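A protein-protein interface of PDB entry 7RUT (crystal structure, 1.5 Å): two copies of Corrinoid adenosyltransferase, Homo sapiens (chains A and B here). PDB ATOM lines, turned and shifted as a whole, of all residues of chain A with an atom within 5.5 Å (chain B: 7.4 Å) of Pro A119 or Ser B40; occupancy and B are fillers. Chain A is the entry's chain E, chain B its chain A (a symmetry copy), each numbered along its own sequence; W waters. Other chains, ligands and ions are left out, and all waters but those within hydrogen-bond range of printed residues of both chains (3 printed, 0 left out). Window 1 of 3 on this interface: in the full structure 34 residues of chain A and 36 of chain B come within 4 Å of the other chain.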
ATOM      1  N   ILE A 117      -6.339   0.692 -28.672  1.00  0.00           N
ATOM      2  CA  ILE A 117      -5.109   0.113 -28.157  1.00  0.00           C
ATOM      3  C   ILE A 117      -5.009   0.401 -26.667  1.00  0.00           C
ATOM      4  O   ILE A 117      -5.492   1.425 -26.161  1.00  0.00           O
ATOM      5  CB  ILE A 117      -3.869   0.629 -28.918  1.00  0.00           C
ATOM      6  CG1 ILE A 117      -3.825   2.156 -28.892  1.00  0.00           C
ATOM      7  CG2 ILE A 117      -3.853   0.088 -30.360  1.00  0.00           C
ATOM      8  CD1 ILE A 117      -2.414   2.720 -28.949  1.00  0.00           C
ATOM      9  N   LEU A 118      -4.416  -0.547 -25.953  1.00  0.00           N
ATOM     10  CA  LEU A 118      -4.000  -0.364 -24.575  1.00  0.00           C
ATOM     11  C   LEU A 118      -2.643   0.322 -24.566  1.00  0.00           C
ATOM     12  O   LEU A 118      -1.926   0.289 -25.566  1.00  0.00           O
ATOM     13  CB  LEU A 118      -3.913  -1.718 -23.870  1.00  0.00           C
ATOM     14  CG  LEU A 118      -5.137  -2.628 -24.000  1.00  0.00           C
ATOM     15  CD1 LEU A 118      -4.854  -4.032 -23.446  1.00  0.00           C
ATOM     16  CD2 LEU A 118      -6.341  -2.009 -23.314  1.00  0.00           C
ATOM     17  N   PRO A 119      -2.269   0.964 -23.458  1.00  0.00           N
ATOM     18  CA  PRO A 119      -0.894   1.462 -23.333  1.00  0.00           C
ATOM     19  C   PRO A 119       0.075   0.299 -23.455  1.00  0.00           C
ATOM     20  O   PRO A 119       0.125  -0.574 -22.584  1.00  0.00           O
ATOM     21  CB  PRO A 119      -0.869   2.099 -21.934  1.00  0.00           C
ATOM     22  CG  PRO A 119      -2.322   2.359 -21.605  1.00  0.00           C
ATOM     23  CD  PRO A 119      -3.084   1.263 -22.265  1.00  0.00           C
ATOM     24  N   SER A 120       0.835   0.278 -24.552  1.00  0.00           N
ATOM     25  CA  SER A 120       1.598  -0.900 -24.942  1.00  0.00           C
ATOM     26  C   SER A 120       2.445  -0.554 -26.153  1.00  0.00           C
ATOM     27  O   SER A 120       2.504   0.616 -26.552  1.00  0.00           O
ATOM     28  CB  SER A 120       0.658  -2.065 -25.261  1.00  0.00           C
ATOM     29  OG  SER A 120      -0.162  -1.760 -26.381  1.00  0.00           O
ATOM     30  N   GLY A 121       3.102  -1.553 -26.741  1.00  0.00           N
ATOM     31  CA  GLY A 121       3.842  -1.377 -27.976  1.00  0.00           C
ATOM     32  C   GLY A 121       5.357  -1.399 -27.868  1.00  0.00           C
ATOM     33  O   GLY A 121       6.028  -1.010 -28.834  1.00  0.00           O
ATOM     34  N   SER A 126       5.504   2.305 -24.487  1.00  0.00           N
ATOM     35  CA  SER A 126       4.815   2.308 -23.204  1.00  0.00           C
ATOM     36  C   SER A 126       5.283   3.468 -22.340  1.00  0.00           C
ATOM     37  O   SER A 126       4.473   4.107 -21.651  1.00  0.00           O
ATOM     38  CB  SER A 126       5.023   0.973 -22.495  1.00  0.00           C
ATOM     39  OG  SER A 126       4.317  -0.052 -23.180  1.00  0.00           O
ATOM     40  N   HIS A 129       3.421   6.432 -23.589  1.00  0.00           N
ATOM     41  CA  HIS A 129       2.044   6.458 -23.106  1.00  0.00           C
ATOM     42  C   HIS A 129       1.966   6.924 -21.661  1.00  0.00           C
ATOM     43  O   HIS A 129       0.989   7.579 -21.277  1.00  0.00           O
ATOM     44  CB  HIS A 129       1.400   5.085 -23.238  1.00  0.00           C
ATOM     45  CG  HIS A 129       0.909   4.801 -24.614  1.00  0.00           C
ATOM     46  ND1 HIS A 129      -0.057   5.566 -25.231  1.00  0.00           N
ATOM     47  CD2 HIS A 129       1.284   3.860 -25.515  1.00  0.00           C
ATOM     48  CE1 HIS A 129      -0.273   5.091 -26.448  1.00  0.00           C
ATOM     49  NE2 HIS A 129       0.533   4.059 -26.646  1.00  0.00           N
ATOM     50  N   PHE A 130       2.966   6.587 -20.845  1.00  0.00           N
ATOM     51  CA  PHE A 130       2.998   7.129 -19.494  1.00  0.00           C
ATOM     52  C   PHE A 130       3.220   8.643 -19.510  1.00  0.00           C
ATOM     53  O   PHE A 130       2.505   9.379 -18.814  1.00  0.00           O
ATOM     54  CB  PHE A 130       4.062   6.410 -18.660  1.00  0.00           C
ATOM     55  CG  PHE A 130       4.108   6.887 -17.234  1.00  0.00           C
ATOM     56  CD1 PHE A 130       3.123   6.517 -16.327  1.00  0.00           C
ATOM     57  CD2 PHE A 130       5.110   7.746 -16.814  1.00  0.00           C
ATOM     58  CE1 PHE A 130       3.142   6.991 -15.010  1.00  0.00           C
ATOM     59  CE2 PHE A 130       5.146   8.212 -15.501  1.00  0.00           C
ATOM     60  CZ  PHE A 130       4.157   7.834 -14.604  1.00  0.00           C
ATOM     61  N   ARG A 132       2.313  10.589 -21.875  1.00  0.00           N
ATOM     62  CA  ARG A 132       1.030  11.114 -22.340  1.00  0.00           C
ATOM     63  C   ARG A 132       0.065  11.297 -21.170  1.00  0.00           C
ATOM     64  O   ARG A 132      -0.603  12.333 -21.052  1.00  0.00           O
ATOM     65  CB  ARG A 132       0.448  10.169 -23.394  1.00  0.00           C
ATOM     66  CG  ARG A 132      -0.896  10.591 -23.993  1.00  0.00           C
ATOM     67  CD  ARG A 132      -1.518   9.413 -24.777  1.00  0.00           C
ATOM     68  NE  ARG A 132      -1.424   8.211 -23.962  1.00  0.00           N
ATOM     69  CZ  ARG A 132      -2.237   7.942 -22.945  1.00  0.00           C
ATOM     70  NH1 ARG A 132      -3.250   8.758 -22.673  1.00  0.00           N
ATOM     71  NH2 ARG A 132      -2.059   6.849 -22.213  1.00  0.00           N
ATOM     72  N   ALA A 133      -0.012  10.304 -20.281  1.00  0.00           N
ATOM     73  CA  ALA A 133      -0.940  10.407 -19.154  1.00  0.00           C
ATOM     74  C   ALA A 133      -0.495  11.489 -18.174  1.00  0.00           C
ATOM     75  O   ALA A 133      -1.330  12.245 -17.642  1.00  0.00           O
ATOM     76  CB  ALA A 133      -1.063   9.043 -18.461  1.00  0.00           C
ATOM     77  N   GLY B  33      -8.364  10.289 -15.817  1.00  0.00           N
ATOM     78  CA  GLY B  33      -6.964  10.480 -16.160  1.00  0.00           C
ATOM     79  C   GLY B  33      -6.040   9.675 -15.278  1.00  0.00           C
ATOM     80  O   GLY B  33      -5.049   9.112 -15.756  1.00  0.00           O
ATOM     81  N   THR B  34      -6.342   9.609 -13.973  1.00  0.00           N
ATOM     82  CA  THR B  34      -5.468   8.857 -13.075  1.00  0.00           C
ATOM     83  C   THR B  34      -5.590   7.353 -13.325  1.00  0.00           C
ATOM     84  O   THR B  34      -4.608   6.614 -13.189  1.00  0.00           O
ATOM     85  CB  THR B  34      -5.777   9.223 -11.615  1.00  0.00           C
ATOM     86  OG1 THR B  34      -5.662  10.645 -11.449  1.00  0.00           O
ATOM     87  CG2 THR B  34      -4.781   8.556 -10.688  1.00  0.00           C
ATOM     88  N   THR B  35      -6.766   6.892 -13.748  1.00  0.00           N
ATOM     89  CA  THR B  35      -6.916   5.493 -14.138  1.00  0.00           C
ATOM     90  C   THR B  35      -6.078   5.182 -15.372  1.00  0.00           C
ATOM     91  O   THR B  35      -5.445   4.116 -15.454  1.00  0.00           O
ATOM     92  CB  THR B  35      -8.397   5.186 -14.379  1.00  0.00           C
ATOM     93  OG1 THR B  35      -9.107   5.335 -13.142  1.00  0.00           O
ATOM     94  CG2 THR B  35      -8.568   3.764 -14.880  1.00  0.00           C
ATOM     95  N   ASP B  36      -6.052   6.107 -16.334  1.00  0.00           N
ATOM     96  CA  ASP B  36      -5.204   5.956 -17.515  1.00  0.00           C
ATOM     97  C   ASP B  36      -3.724   5.981 -17.144  1.00  0.00           C
ATOM     98  O   ASP B  36      -2.909   5.246 -17.725  1.00  0.00           O
ATOM     99  CB  ASP B  36      -5.519   7.072 -18.504  1.00  0.00           C
ATOM    100  CG  ASP B  36      -4.571   7.093 -19.689  1.00  0.00           C
ATOM    101  OD1 ASP B  36      -4.329   6.021 -20.296  1.00  0.00           O
ATOM    102  OD2 ASP B  36      -4.087   8.189 -20.030  1.00  0.00           O
ATOM    103  N   GLU B  37      -3.352   6.844 -16.197  1.00  0.00           N
ATOM    104  CA  GLU B  37      -1.973   6.865 -15.716  1.00  0.00           C
ATOM    105  C   GLU B  37      -1.580   5.521 -15.114  1.00  0.00           C
ATOM    106  O   GLU B  37      -0.478   5.014 -15.374  1.00  0.00           O
ATOM    107  CB  GLU B  37      -1.792   8.006 -14.703  1.00  0.00           C
ATOM    108  CG  GLU B  37      -0.350   8.299 -14.338  1.00  0.00           C
ATOM    109  CD  GLU B  37      -0.190   9.500 -13.414  1.00  0.00           C
ATOM    110  OE1 GLU B  37      -1.158  10.285 -13.214  1.00  0.00           O
ATOM    111  OE2 GLU B  37       0.923   9.653 -12.875  1.00  0.00           O
ATOM    112  N   LEU B  38      -2.474   4.921 -14.321  1.00  0.00           N
ATOM    113  CA  LEU B  38      -2.225   3.592 -13.767  1.00  0.00           C
ATOM    114  C   LEU B  38      -2.066   2.553 -14.871  1.00  0.00           C
ATOM    115  O   LEU B  38      -1.136   1.737 -14.842  1.00  0.00           O
ATOM    116  CB  LEU B  38      -3.375   3.200 -12.830  1.00  0.00           C
ATOM    117  CG  LEU B  38      -3.376   1.739 -12.350  1.00  0.00           C
ATOM    118  CD1 LEU B  38      -2.104   1.380 -11.546  1.00  0.00           C
ATOM    119  CD2 LEU B  38      -4.646   1.456 -11.558  1.00  0.00           C
ATOM    120  N   SER B  39      -2.973   2.556 -15.845  1.00  0.00           N
ATOM    121  CA  SER B  39      -2.860   1.579 -16.924  1.00  0.00           C
ATOM    122  C   SER B  39      -1.552   1.753 -17.679  1.00  0.00           C
ATOM    123  O   SER B  39      -0.933   0.767 -18.110  1.00  0.00           O
ATOM    124  CB  SER B  39      -4.038   1.694 -17.889  1.00  0.00           C
ATOM    125  OG  SER B  39      -3.931   0.646 -18.860  1.00  0.00           O
ATOM    126  N   SER B  40      -1.106   2.992 -17.835  1.00  0.00           N
ATOM    127  CA  SER B  40       0.132   3.256 -18.566  1.00  0.00           C
ATOM    128  C   SER B  40       1.344   2.787 -17.769  1.00  0.00           C
ATOM    129  O   SER B  40       2.294   2.221 -18.336  1.00  0.00           O
ATOM    130  CB  SER B  40       0.218   4.749 -18.862  1.00  0.00           C
ATOM    131  OG  SER B  40      -0.781   5.094 -19.813  1.00  0.00           O
ATOM    132  N   ALA B  41       1.325   3.006 -16.455  1.00  0.00           N
ATOM    133  CA  ALA B  41       2.383   2.492 -15.598  1.00  0.00           C
ATOM    134  C   ALA B  41       2.443   0.975 -15.667  1.00  0.00           C
ATOM    135  O   ALA B  41       3.535   0.392 -15.746  1.00  0.00           O
ATOM    136  CB  ALA B  41       2.164   2.968 -14.162  1.00  0.00           C
ATOM    137  N   ILE B  42       1.273   0.322 -15.676  1.00  0.00           N
ATOM    138  CA  ILE B  42       1.232  -1.132 -15.792  1.00  0.00           C
ATOM    139  C   ILE B  42       1.773  -1.567 -17.145  1.00  0.00           C
ATOM    140  O   ILE B  42       2.466  -2.586 -17.252  1.00  0.00           O
ATOM    141  CB  ILE B  42      -0.197  -1.657 -15.553  1.00  0.00           C
ATOM    142  CG1 ILE B  42      -0.572  -1.512 -14.073  1.00  0.00           C
ATOM    143  CG2 ILE B  42      -0.302  -3.124 -15.984  1.00  0.00           C
ATOM    144  CD1 ILE B  42      -2.039  -1.766 -13.759  1.00  0.00           C
ATOM    145  N   GLY B  43       1.471  -0.800 -18.196  1.00  0.00           N
ATOM    146  CA  GLY B  43       1.974  -1.140 -19.518  1.00  0.00           C
ATOM    147  C   GLY B  43       3.493  -1.146 -19.570  1.00  0.00           C
ATOM    148  O   GLY B  43       4.104  -2.012 -20.204  1.00  0.00           O
ATOM    149  N   PHE B  44       4.127  -0.192 -18.889  1.00  0.00           N
ATOM    150  CA  PHE B  44       5.587  -0.188 -18.843  1.00  0.00           C
ATOM    151  C   PHE B  44       6.113  -1.362 -18.024  1.00  0.00           C
ATOM    152  O   PHE B  44       7.054  -2.047 -18.442  1.00  0.00           O
ATOM    153  CB  PHE B  44       6.099   1.136 -18.285  1.00  0.00           C
ATOM    154  CG  PHE B  44       7.595   1.242 -18.293  1.00  0.00           C
ATOM    155  CD1 PHE B  44       8.272   1.551 -19.461  1.00  0.00           C
ATOM    156  CD2 PHE B  44       8.323   1.000 -17.139  1.00  0.00           C
ATOM    157  CE1 PHE B  44       9.663   1.639 -19.481  1.00  0.00           C
ATOM    158  CE2 PHE B  44       9.710   1.080 -17.140  1.00  0.00           C
ATOM    159  CZ  PHE B  44      10.386   1.399 -18.320  1.00  0.00           C
ATOM    160  N   ALA B  45       5.507  -1.625 -16.864  1.00  0.00           N
ATOM    161  CA  ALA B  45       5.895  -2.786 -16.071  1.00  0.00           C
ATOM    162  C   ALA B  45       5.729  -4.072 -16.872  1.00  0.00           C
ATOM    163  O   ALA B  45       6.547  -4.993 -16.757  1.00  0.00           O
ATOM    164  CB  ALA B  45       5.079  -2.840 -14.779  1.00  0.00           C
ATOM    165  N   LEU B  46       4.687  -4.132 -17.708  1.00  0.00           N
ATOM    166  CA  LEU B  46       4.437  -5.308 -18.540  1.00  0.00           C
ATOM    167  C   LEU B  46       5.588  -5.542 -19.506  1.00  0.00           C
ATOM    168  O   LEU B  46       5.961  -6.693 -19.781  1.00  0.00           O
ATOM    169  CB  LEU B  46       3.110  -5.120 -19.294  1.00  0.00           C
ATOM    170  CG  LEU B  46       2.435  -6.323 -19.936  1.00  0.00           C
ATOM    171  CD1 LEU B  46       2.582  -7.482 -19.002  1.00  0.00           C
ATOM    172  CD2 LEU B  46       0.952  -6.043 -20.239  1.00  0.00           C
ATOM    173  N   GLU B  47       6.187  -4.464 -20.013  1.00  0.00           N
ATOM    174  CA  GLU B  47       7.313  -4.635 -20.927  1.00  0.00           C
ATOM    175  C   GLU B  47       8.512  -5.258 -20.224  1.00  0.00           C
ATOM    176  O   GLU B  47       9.282  -5.991 -20.855  1.00  0.00           O
ATOM    177  CB  GLU B  47       7.705  -3.296 -21.559  1.00  0.00           C
ATOM    178  CG  GLU B  47       6.574  -2.591 -22.310  1.00  0.00           C
ATOM    179  CD  GLU B  47       6.220  -3.269 -23.625  1.00  0.00           C
ATOM    180  OE1 GLU B  47       7.055  -4.040 -24.140  1.00  0.00           O
ATOM    181  OE2 GLU B  47       5.108  -3.022 -24.146  1.00  0.00           O
ATOM    182  N   GLN B  64      -5.379  -4.325 -17.616  1.00  0.00           N
ATOM    183  CA  GLN B  64      -5.494  -3.122 -18.441  1.00  0.00           C
ATOM    184  C   GLN B  64      -6.842  -3.060 -19.153  1.00  0.00           C
ATOM    185  O   GLN B  64      -7.418  -1.976 -19.314  1.00  0.00           O
ATOM    186  CB  GLN B  64      -4.369  -3.066 -19.462  1.00  0.00           C
ATOM    187  CG  GLN B  64      -2.996  -2.832 -18.871  1.00  0.00           C
ATOM    188  CD  GLN B  64      -1.980  -2.649 -19.962  1.00  0.00           C
ATOM    189  OE1 GLN B  64      -1.695  -3.580 -20.715  1.00  0.00           O
ATOM    190  NE2 GLN B  64      -1.460  -1.436 -20.097  1.00  0.00           N
ATOM    191  N   LEU B  67      -9.210  -1.960 -16.671  1.00  0.00           N
ATOM    192  CA  LEU B  67      -9.012  -0.540 -16.362  1.00  0.00           C
ATOM    193  C   LEU B  67      -9.616   0.341 -17.442  1.00  0.00           C
ATOM    194  O   LEU B  67     -10.035   1.474 -17.164  1.00  0.00           O
ATOM    195  CB  LEU B  67      -7.525  -0.211 -16.183  1.00  0.00           C
ATOM    196  CG  LEU B  67      -6.923  -0.698 -14.867  1.00  0.00           C
ATOM    197  CD1 LEU B  67      -5.414  -0.464 -14.850  1.00  0.00           C
ATOM    198  CD2 LEU B  67      -7.599  -0.029 -13.664  1.00  0.00           C
ATOM    199  N   GLN B  68      -9.699  -0.152 -18.678  1.00  0.00           N
ATOM    200  CA  GLN B  68     -10.433   0.618 -19.666  1.00  0.00           C
ATOM    201  C   GLN B  68     -11.924   0.646 -19.348  1.00  0.00           C
ATOM    202  O   GLN B  68     -12.588   1.677 -19.528  1.00  0.00           O
ATOM    203  CB  GLN B  68     -10.191   0.085 -21.072  1.00  0.00           C
ATOM    204  CG  GLN B  68     -10.926   0.960 -22.047  1.00  0.00           C
ATOM    205  CD  GLN B  68     -10.364   2.397 -22.093  1.00  0.00           C
ATOM    206  OE1 GLN B  68     -10.001   3.004 -21.079  1.00  0.00           O
ATOM    207  NE2 GLN B  68     -10.389   2.966 -23.258  1.00  0.00           N
ATOM    208  N   CYS B 131       3.432   0.992  -9.608  1.00  0.00           N
ATOM    209  CA  CYS B 131       2.064   0.787 -10.085  1.00  0.00           C
ATOM    210  C   CYS B 131       1.077   0.753  -8.928  1.00  0.00           C
ATOM    211  O   CYS B 131      -0.005   1.353  -8.998  1.00  0.00           O
ATOM    212  CB  CYS B 131       1.985  -0.524 -10.873  1.00  0.00           C
ATOM    213  SG  CYS B 131       2.831  -0.416 -12.460  1.00  0.00           S
ATOM    214  N   VAL B 134       0.429   4.230  -7.667  1.00  0.00           N
ATOM    215  CA  VAL B 134      -0.442   4.979  -8.571  1.00  0.00           C
ATOM    216  C   VAL B 134      -1.872   4.463  -8.478  1.00  0.00           C
ATOM    217  O   VAL B 134      -2.833   5.236  -8.578  1.00  0.00           O
ATOM    218  CB  VAL B 134       0.090   4.910 -10.018  1.00  0.00           C
ATOM    219  CG1 VAL B 134      -0.846   5.638 -10.974  1.00  0.00           C
ATOM    220  CG2 VAL B 134       1.486   5.508 -10.099  1.00  0.00           C
HETATM  221  O   HOH W   1      -3.894  11.814 -16.840  1.00  0.00           O
HETATM  222  O   HOH W   2       0.311  -3.440 -22.273  1.00  0.00           O
HETATM  223  O   HOH W   3       2.290   2.437 -21.083  1.00  0.00           O
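The guanidinium group of Arg A132 lies within salt-bridge range of the side-chain carboxylate of Asp B36 (2.8 Å).
OG of Ser A126 sits at hydrogen-bond distance from OE2 of Glu B47, 3.2 Å away.
The guanidinium group (NH2) of Arg A132 is in hydrogen-bond range of the side-chain hydroxyl (OG) of Ser B40 (3.2 Å).
The side-chain amide nitrogen of Gln B64 is in hydrogen-bond range of the backbone carbonyl oxygen of Pro A119, 3.1 Å away.
The backbone carbonyl oxygen of His A129 is in hydrogen-bond range of the side-chain hydroxyl of Ser B40, 3.4 Å away.
The side-chain amide nitrogen (NE2) of Gln B64 is in hydrogen-bond range of the backbone carbonyl oxygen (O) of Ser B39 (3.0 Å).
The backbone carbonyl oxygen (O) of Asp B36 sits at hydrogen-bond distance from the side-chain hydroxyl (OG) of Ser B40 (3.0 Å).
The backbone carbonyl oxygen (O) of Ala B41 sits at hydrogen-bond distance from the side-chain sulfur (SG) of Cys B131 (3.5 Å).
The guanidinium group of Arg A132 sits at hydrogen-bond distance from a ring nitrogen (ND1) of His A129 (3.2 Å).
Hydrophobic or aromatic side chains of chain A within 4 Å of the printed part of chain B: Pro A119, Phe A130 and Ala A133.
Among the printed residues, pairs that only touch across the chains: Ala A133 with Asp B36 (3.5 Å), Pro A119 with Ser B39 (3.6 Å), Ser A126 with Gly B43 (3.6 Å), Gly A121 with Glu B47 (3.6 Å), Pro A119 with Ser B40 (3.6 Å), Ala A133 with Glu B37 (3.6 Å), Pro A119 with Gly B43 (3.6 Å), Phe A130 with Ser B40 (3.7 Å), Phe A130 with Glu B37 (3.8 Å), Ser A126 with Phe B44 (3.9 Å) and Phe A130 with Ala B41 (3.9 Å).
Water W2 lies within hydrogen-bond range of OE1 of Gln B64 (2.5 Å) and O of Pro A119 (2.9 Å).
Water W1 lies within hydrogen-bond range of the backbone carbonyl oxygen (O) of Ala A133 (2.7 Å) and the backbone carbonyl oxygen (O) of Gly B33 (3.1 Å).
Water W3 lies within hydrogen-bond range of the backbone carbonyl oxygen of Ser B40 (2.8 Å) and the backbone carbonyl oxygen of Ser A126 (2.8 Å).
No position is printed for both chains.
Of the 16 pairs that touch across the chains among the printed residues, none has its exchanged pair printed and touching as well.
Of chain B, only Ser B39, Ser B40, Gly B43 and Gln B64 come within 4 Å of Pro A119.
Ser B40 touches just these residues of chain A: Pro A119 (3.6 Å), His A129 (3.4 Å), Phe A130 (3.7 Å) and Arg A132 (3.2 Å).
Printed residues of chain B within 4 Å of Gly A121: Glu B47.
Printed residues of chain A within 4 Å of Ser B39: Pro A119.
Printed residues of chain A within 4 Å of Gln B64: Pro A119.
Printed residues of chain B within 4 Å of Ala A133: Asp B36 (3.5 Å) and Glu B37 (3.6 Å).
The nearest residue of chain B that does not touch Pro A119 is Asp B36 (4.4 Å).
The nearest residue of chain A that does not touch Ser B40 is Ala A133 (4.2 Å).
The nearest printed residue of chain A that does not touch Ala B41 is Pro A119 (6.0 Å).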
